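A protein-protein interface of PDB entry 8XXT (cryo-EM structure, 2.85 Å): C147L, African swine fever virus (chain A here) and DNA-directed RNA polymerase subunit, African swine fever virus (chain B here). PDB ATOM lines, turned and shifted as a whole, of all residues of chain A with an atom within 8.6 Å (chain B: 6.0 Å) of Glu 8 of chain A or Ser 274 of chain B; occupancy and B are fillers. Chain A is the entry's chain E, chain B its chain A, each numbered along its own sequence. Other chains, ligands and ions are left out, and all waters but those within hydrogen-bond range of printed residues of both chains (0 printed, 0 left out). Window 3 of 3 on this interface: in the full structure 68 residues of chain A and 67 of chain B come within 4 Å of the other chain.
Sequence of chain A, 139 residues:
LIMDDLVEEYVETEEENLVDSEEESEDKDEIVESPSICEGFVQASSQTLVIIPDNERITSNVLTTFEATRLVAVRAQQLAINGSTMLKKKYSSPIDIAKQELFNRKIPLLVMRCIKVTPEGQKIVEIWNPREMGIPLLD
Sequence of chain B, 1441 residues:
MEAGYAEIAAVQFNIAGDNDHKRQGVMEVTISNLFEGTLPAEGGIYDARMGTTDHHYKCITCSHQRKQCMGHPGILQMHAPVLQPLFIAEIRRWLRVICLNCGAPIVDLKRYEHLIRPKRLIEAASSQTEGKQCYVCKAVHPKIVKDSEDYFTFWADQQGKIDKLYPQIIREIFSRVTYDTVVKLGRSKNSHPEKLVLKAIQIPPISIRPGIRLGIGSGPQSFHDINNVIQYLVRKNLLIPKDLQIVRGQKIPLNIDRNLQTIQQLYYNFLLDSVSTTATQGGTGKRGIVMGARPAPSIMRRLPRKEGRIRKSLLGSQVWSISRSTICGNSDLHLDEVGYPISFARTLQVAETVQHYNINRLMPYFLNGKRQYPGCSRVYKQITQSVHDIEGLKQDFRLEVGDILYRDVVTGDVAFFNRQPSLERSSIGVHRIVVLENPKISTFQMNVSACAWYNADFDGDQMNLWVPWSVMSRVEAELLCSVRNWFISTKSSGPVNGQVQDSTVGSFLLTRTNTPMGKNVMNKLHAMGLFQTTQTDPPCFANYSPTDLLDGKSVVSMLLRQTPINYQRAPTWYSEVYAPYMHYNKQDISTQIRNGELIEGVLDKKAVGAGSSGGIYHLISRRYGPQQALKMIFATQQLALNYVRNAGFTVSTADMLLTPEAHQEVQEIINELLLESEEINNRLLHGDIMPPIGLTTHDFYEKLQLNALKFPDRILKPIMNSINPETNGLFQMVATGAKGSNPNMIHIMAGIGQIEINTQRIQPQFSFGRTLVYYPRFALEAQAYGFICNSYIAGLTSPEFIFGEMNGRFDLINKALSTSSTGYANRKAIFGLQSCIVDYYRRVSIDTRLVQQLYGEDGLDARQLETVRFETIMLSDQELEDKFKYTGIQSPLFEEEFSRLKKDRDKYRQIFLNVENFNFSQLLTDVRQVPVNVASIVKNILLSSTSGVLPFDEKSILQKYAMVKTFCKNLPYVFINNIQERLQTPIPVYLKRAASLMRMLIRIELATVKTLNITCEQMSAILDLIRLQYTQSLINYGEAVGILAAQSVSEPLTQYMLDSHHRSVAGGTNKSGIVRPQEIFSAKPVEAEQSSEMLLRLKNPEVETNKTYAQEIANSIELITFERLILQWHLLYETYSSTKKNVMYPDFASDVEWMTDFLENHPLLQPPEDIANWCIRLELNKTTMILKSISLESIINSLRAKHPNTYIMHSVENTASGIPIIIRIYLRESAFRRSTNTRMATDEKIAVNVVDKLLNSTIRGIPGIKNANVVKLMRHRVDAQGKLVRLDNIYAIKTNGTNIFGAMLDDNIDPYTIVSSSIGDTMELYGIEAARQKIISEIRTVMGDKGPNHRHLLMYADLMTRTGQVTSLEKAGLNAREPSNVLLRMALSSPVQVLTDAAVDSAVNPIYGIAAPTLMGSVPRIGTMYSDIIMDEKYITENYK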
ATOM      1  N   ASP A   5     -20.537  22.392  32.438  1.00  0.00           N
ATOM      2  CA  ASP A   5     -19.618  22.391  31.297  1.00  0.00           C
ATOM      3  C   ASP A   5     -20.393  22.297  29.981  1.00  0.00           C
ATOM      4  O   ASP A   5     -20.180  21.405  29.157  1.00  0.00           O
ATOM      5  CB  ASP A   5     -18.581  21.265  31.415  1.00  0.00           C
ATOM      6  CG  ASP A   5     -17.763  21.356  32.689  1.00  0.00           C
ATOM      7  OD1 ASP A   5     -17.330  22.472  33.045  1.00  0.00           O
ATOM      8  OD2 ASP A   5     -17.549  20.308  33.334  1.00  0.00           O
ATOM      9  N   LEU A   6     -21.308  23.246  29.802  1.00  0.00           N
ATOM     10  CA  LEU A   6     -22.136  23.285  28.608  1.00  0.00           C
ATOM     11  C   LEU A   6     -21.314  23.699  27.390  1.00  0.00           C
ATOM     12  O   LEU A   6     -20.279  24.364  27.494  1.00  0.00           O
ATOM     13  CB  LEU A   6     -23.314  24.241  28.798  1.00  0.00           C
ATOM     14  CG  LEU A   6     -24.327  23.881  29.887  1.00  0.00           C
ATOM     15  CD1 LEU A   6     -23.933  24.472  31.234  1.00  0.00           C
ATOM     16  CD2 LEU A   6     -25.718  24.342  29.484  1.00  0.00           C
ATOM     17  N   VAL A   7     -21.802  23.303  26.215  1.00  0.00           N
ATOM     18  CA  VAL A   7     -21.099  23.530  24.957  1.00  0.00           C
ATOM     19  C   VAL A   7     -21.453  24.919  24.434  1.00  0.00           C
ATOM     20  O   VAL A   7     -21.085  25.289  23.313  1.00  0.00           O
ATOM     21  CB  VAL A   7     -21.441  22.426  23.938  1.00  0.00           C
ATOM     22  CG1 VAL A   7     -22.870  22.582  23.429  1.00  0.00           C
ATOM     23  CG2 VAL A   7     -20.429  22.388  22.793  1.00  0.00           C
ATOM     24  N   GLU A   8     -22.167  25.697  25.252  1.00  0.00           N
ATOM     25  CA  GLU A   8     -22.552  27.066  24.923  1.00  0.00           C
ATOM     26  C   GLU A   8     -23.450  27.112  23.695  1.00  0.00           C
ATOM     27  O   GLU A   8     -24.144  26.141  23.379  1.00  0.00           O
ATOM     28  CB  GLU A   8     -21.320  27.946  24.689  1.00  0.00           C
ATOM     29  CG  GLU A   8     -20.286  27.911  25.797  1.00  0.00           C
ATOM     30  CD  GLU A   8     -19.077  28.772  25.482  1.00  0.00           C
ATOM     31  OE1 GLU A   8     -19.195  29.671  24.623  1.00  0.00           O
ATOM     32  OE2 GLU A   8     -18.009  28.548  26.088  1.00  0.00           O
ATOM     33  N   GLU A   9     -23.439  28.249  23.005  1.00  0.00           N
ATOM     34  CA  GLU A   9     -24.165  28.452  21.761  1.00  0.00           C
ATOM     35  C   GLU A   9     -23.442  29.539  20.987  1.00  0.00           C
ATOM     36  O   GLU A   9     -22.786  30.392  21.589  1.00  0.00           O
ATOM     37  CB  GLU A   9     -25.625  28.846  22.023  1.00  0.00           C
ATOM     38  CG  GLU A   9     -26.626  28.251  21.042  1.00  0.00           C
ATOM     39  CD  GLU A   9     -26.772  29.073  19.777  1.00  0.00           C
ATOM     40  OE1 GLU A   9     -26.146  30.150  19.690  1.00  0.00           O
ATOM     41  OE2 GLU A   9     -27.517  28.646  18.872  1.00  0.00           O
ATOM     42  N   TYR A  10     -23.554  29.503  19.662  1.00  0.00           N
ATOM     43  CA  TYR A  10     -22.788  30.399  18.808  1.00  0.00           C
ATOM     44  C   TYR A  10     -23.714  31.082  17.814  1.00  0.00           C
ATOM     45  O   TYR A  10     -24.511  30.418  17.147  1.00  0.00           O
ATOM     46  CB  TYR A  10     -21.681  29.630  18.085  1.00  0.00           C
ATOM     47  CG  TYR A  10     -21.014  30.414  16.992  1.00  0.00           C
ATOM     48  CD1 TYR A  10     -20.301  31.569  17.277  1.00  0.00           C
ATOM     49  CD2 TYR A  10     -21.078  29.991  15.676  1.00  0.00           C
ATOM     50  CE1 TYR A  10     -19.682  32.287  16.279  1.00  0.00           C
ATOM     51  CE2 TYR A  10     -20.463  30.698  14.678  1.00  0.00           C
ATOM     52  CZ  TYR A  10     -19.767  31.846  14.980  1.00  0.00           C
ATOM     53  OH  TYR A  10     -19.150  32.558  13.981  1.00  0.00           O
ATOM     54  N   VAL A  11     -23.596  32.404  17.711  1.00  0.00           N
ATOM     55  CA  VAL A  11     -24.508  33.230  16.928  1.00  0.00           C
ATOM     56  C   VAL A  11     -23.702  34.084  15.958  1.00  0.00           C
ATOM     57  O   VAL A  11     -22.698  34.695  16.339  1.00  0.00           O
ATOM     58  CB  VAL A  11     -25.382  34.117  17.840  1.00  0.00           C
ATOM     59  CG1 VAL A  11     -25.797  35.394  17.126  1.00  0.00           C
ATOM     60  CG2 VAL A  11     -26.602  33.356  18.319  1.00  0.00           C
ATOM     61  N   GLU A  12     -24.143  34.117  14.703  1.00  0.00           N
ATOM     62  CA  GLU A  12     -23.578  34.979  13.672  1.00  0.00           C
ATOM     63  C   GLU A  12     -24.629  36.006  13.273  1.00  0.00           C
ATOM     64  O   GLU A  12     -25.743  35.636  12.889  1.00  0.00           O
ATOM     65  CB  GLU A  12     -23.144  34.159  12.459  1.00  0.00           C
ATOM     66  CG  GLU A  12     -22.569  32.800  12.806  1.00  0.00           C
ATOM     67  CD  GLU A  12     -21.690  32.246  11.707  1.00  0.00           C
ATOM     68  OE1 GLU A  12     -22.124  32.270  10.542  1.00  0.00           O
ATOM     69  OE2 GLU A  12     -20.564  31.796  11.995  1.00  0.00           O
ATOM     70  N   LEU B 272     -25.335  21.283  11.918  1.00  0.00           N
ATOM     71  CA  LEU B 272     -25.556  22.634  12.418  1.00  0.00           C
ATOM     72  C   LEU B 272     -26.064  22.667  13.855  1.00  0.00           C
ATOM     73  O   LEU B 272     -26.786  23.596  14.227  1.00  0.00           O
ATOM     74  CB  LEU B 272     -26.527  23.377  11.503  1.00  0.00           C
ATOM     75  CG  LEU B 272     -25.976  23.811  10.149  1.00  0.00           C
ATOM     76  CD1 LEU B 272     -27.058  24.489   9.345  1.00  0.00           C
ATOM     77  CD2 LEU B 272     -24.800  24.741  10.336  1.00  0.00           C
ATOM     78  N   ASP B 273     -25.710  21.682  14.671  1.00  0.00           N
ATOM     79  CA  ASP B 273     -26.071  21.737  16.081  1.00  0.00           C
ATOM     80  C   ASP B 273     -25.241  22.799  16.784  1.00  0.00           C
ATOM     81  O   ASP B 273     -24.025  22.882  16.586  1.00  0.00           O
ATOM     82  CB  ASP B 273     -25.862  20.377  16.743  1.00  0.00           C
ATOM     83  CG  ASP B 273     -26.388  20.332  18.163  1.00  0.00           C
ATOM     84  OD1 ASP B 273     -27.536  20.763  18.388  1.00  0.00           O
ATOM     85  OD2 ASP B 273     -25.653  19.861  19.057  1.00  0.00           O
ATOM     86  N   SER B 274     -25.903  23.616  17.605  1.00  0.00           N
ATOM     87  CA  SER B 274     -25.279  24.681  18.383  1.00  0.00           C
ATOM     88  C   SER B 274     -24.655  25.764  17.511  1.00  0.00           C
ATOM     89  O   SER B 274     -23.734  26.458  17.952  1.00  0.00           O
ATOM     90  CB  SER B 274     -24.231  24.117  19.351  1.00  0.00           C
ATOM     91  OG  SER B 274     -24.132  24.904  20.523  1.00  0.00           O
ATOM     92  N   VAL B 275     -25.130  25.927  16.279  1.00  0.00           N
ATOM     93  CA  VAL B 275     -24.672  26.980  15.380  1.00  0.00           C
ATOM     94  C   VAL B 275     -25.900  27.723  14.876  1.00  0.00           C
ATOM     95  O   VAL B 275     -26.773  27.122  14.239  1.00  0.00           O
ATOM     96  CB  VAL B 275     -23.858  26.424  14.200  1.00  0.00           C
ATOM     97  CG1 VAL B 275     -23.339  27.558  13.338  1.00  0.00           C
ATOM     98  CG2 VAL B 275     -22.713  25.563  14.700  1.00  0.00           C
ATOM     99  N   SER B 276     -25.975  29.023  15.160  1.00  0.00           N
ATOM    100  CA  SER B 276     -27.177  29.772  14.810  1.00  0.00           C
ATOM    101  C   SER B 276     -27.158  30.234  13.358  1.00  0.00           C
ATOM    102  O   SER B 276     -27.994  29.807  12.558  1.00  0.00           O
ATOM    103  CB  SER B 276     -27.346  30.965  15.752  1.00  0.00           C
ATOM    104  OG  SER B 276     -27.567  30.529  17.082  1.00  0.00           O
ATOM    105  N   SER B 298     -21.300  19.628  16.567  1.00  0.00           N
ATOM    106  CA  SER B 298     -21.603  19.314  15.185  1.00  0.00           C
ATOM    107  C   SER B 298     -20.397  19.582  14.292  1.00  0.00           C
ATOM    108  O   SER B 298     -19.346  20.049  14.735  1.00  0.00           O
ATOM    109  CB  SER B 298     -22.806  20.123  14.717  1.00  0.00           C
ATOM    110  OG  SER B 298     -22.554  21.510  14.841  1.00  0.00           O
ATOM    111  N   ARG B 301     -19.753  23.266  14.034  1.00  0.00           N
ATOM    112  CA  ARG B 301     -19.333  23.861  15.295  1.00  0.00           C
ATOM    113  C   ARG B 301     -17.824  23.806  15.480  1.00  0.00           C
ATOM    114  O   ARG B 301     -17.279  24.579  16.273  1.00  0.00           O
ATOM    115  CB  ARG B 301     -20.031  23.160  16.459  1.00  0.00           C
ATOM    116  CG  ARG B 301     -19.942  23.894  17.781  1.00  0.00           C
ATOM    117  CD  ARG B 301     -20.335  25.351  17.626  1.00  0.00           C
ATOM    118  NE  ARG B 301     -19.495  26.229  18.430  1.00  0.00           N
ATOM    119  CZ  ARG B 301     -19.734  26.543  19.694  1.00  0.00           C
ATOM    120  NH1 ARG B 301     -20.787  26.066  20.338  1.00  0.00           N
ATOM    121  NH2 ARG B 301     -18.896  27.355  20.331  1.00  0.00           N
ATOM    122  N   ARG B 305     -14.895  30.473  16.308  1.00  0.00           N
ATOM    123  CA  ARG B 305     -14.334  30.841  17.608  1.00  0.00           C
ATOM    124  C   ARG B 305     -12.832  30.599  17.683  1.00  0.00           C
ATOM    125  O   ARG B 305     -12.239  30.011  16.774  1.00  0.00           O
ATOM    126  CB  ARG B 305     -15.044  30.098  18.744  1.00  0.00           C
ATOM    127  CG  ARG B 305     -16.558  30.145  18.665  1.00  0.00           C
ATOM    128  CD  ARG B 305     -17.062  31.575  18.791  1.00  0.00           C
ATOM    129  NE  ARG B 305     -17.101  32.078  20.162  1.00  0.00           N
ATOM    130  CZ  ARG B 305     -17.649  31.460  21.202  1.00  0.00           C
ATOM    131  NH1 ARG B 305     -18.325  30.329  21.067  1.00  0.00           N
ATOM    132  NH2 ARG B 305     -17.540  32.008  22.409  1.00  0.00           N
ATOM    133  N   GLU B 307     -11.083  28.660  19.667  1.00  0.00           N
ATOM    134  CA  GLU B 307     -10.761  27.246  19.781  1.00  0.00           C
ATOM    135  C   GLU B 307     -11.246  26.429  18.591  1.00  0.00           C
ATOM    136  O   GLU B 307     -11.235  25.197  18.659  1.00  0.00           O
ATOM    137  CB  GLU B 307     -11.344  26.680  21.079  1.00  0.00           C
ATOM    138  CG  GLU B 307     -12.862  26.602  21.104  1.00  0.00           C
ATOM    139  CD  GLU B 307     -13.511  27.920  21.484  1.00  0.00           C
ATOM    140  OE1 GLU B 307     -12.792  28.821  21.965  1.00  0.00           O
ATOM    141  OE2 GLU B 307     -14.740  28.056  21.305  1.00  0.00           O
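The backbone carbonyl oxygen of Tyr 10 of chain A lies within hydrogen-bond range of the backbone NH of Ser 276 of chain B (2.8 Å).
The guanidinium group of Arg 305 of chain B is in salt-bridge range of the side-chain carboxylate of Glu 8 of chain A (3.6 Å).
The side-chain hydroxyl (OG) of Ser 276 of chain B is in hydrogen-bond range of the side-chain carboxylate (OE2) of Glu 9 of chain A (2.6 Å).
O of Glu 8 of chain A lies within hydrogen-bond range of OG of Ser 274 of chain B, at 3.1 Å.
The guanidinium group of Arg 301 of chain B lies within hydrogen-bond range of the backbone carbonyl oxygen of Val 7 of chain A, at 3.1 Å.
The backbone carbonyl oxygen of Ser 274 of chain B is in hydrogen-bond range of the backbone NH of Tyr 10 of chain A (3.5 Å).
OE2 of Glu 12 of chain A lies within hydrogen-bond range of OH of Tyr 10 of chain A, 2.6 Å away.
N of Arg 301 of chain B sits at hydrogen-bond distance from OG of Ser 298 of chain B (3.4 Å).
OG of Ser 274 of chain B touches CG1 of Val 7 of chain A (3.9 Å).
OG of Ser 274 of chain B touches CA of Glu 9 of chain A (3.8 Å).
Tyr 10 of chain A touches Val 275 of chain B (O to C, 3.8 Å).
CB of Tyr 10 of chain A touches CZ of Arg 301 of chain B, at 3.99 Å.
Tyr 10 of chain A touches Arg 305 of chain B (CD1 to CD, 3.6 Å).
OG of Ser 276 of chain B touches CG2 of Val 11 of chain A (3.2 Å).
Glu 8 of chain A touches just these residues of chain B: Ser 274 (3.1 Å) and Arg 305 (3.6 Å).
Of the printed residues of chain B, Glu 9 of chain A touches Ser 274 and Ser 276.
Of the printed residues of chain B, Tyr 10 of chain A touches Ser 274, Val 275, Ser 276, Arg 301 and Arg 305.
No residue of chain A comes within 4 Å of Asp 273 of chain B.
Ser 274 of chain B touches just these residues of chain A: Val 7 (3.9 Å), Glu 8 (3.1 Å), Glu 9 (3.8 Å) and Tyr 10 (3.5 Å).
Of the printed residues of chain A, Val 275 of chain B touches Tyr 10.
Of the printed residues of chain A, Ser 276 of chain B touches Glu 9, Tyr 10 and Val 11.
Of the printed residues of chain A, Arg 301 of chain B touches Val 7 and Tyr 10.
The nearest residue of chain B that does not touch Glu 8 of chain A is Arg 301 of chain B (4.4 Å).
Of the 9 printed residues of chain B, 5 touch a printed residue of chain A.
Of the 8 printed residues of chain A, 5 touch a printed residue of chain B.
Among the printed residues, Asp or Glu carboxylates within 4 Å of a Lys or Arg side-chain nitrogen of the other chain: Glu 8 of chain A with Arg 305 of chain B (3.6 Å).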
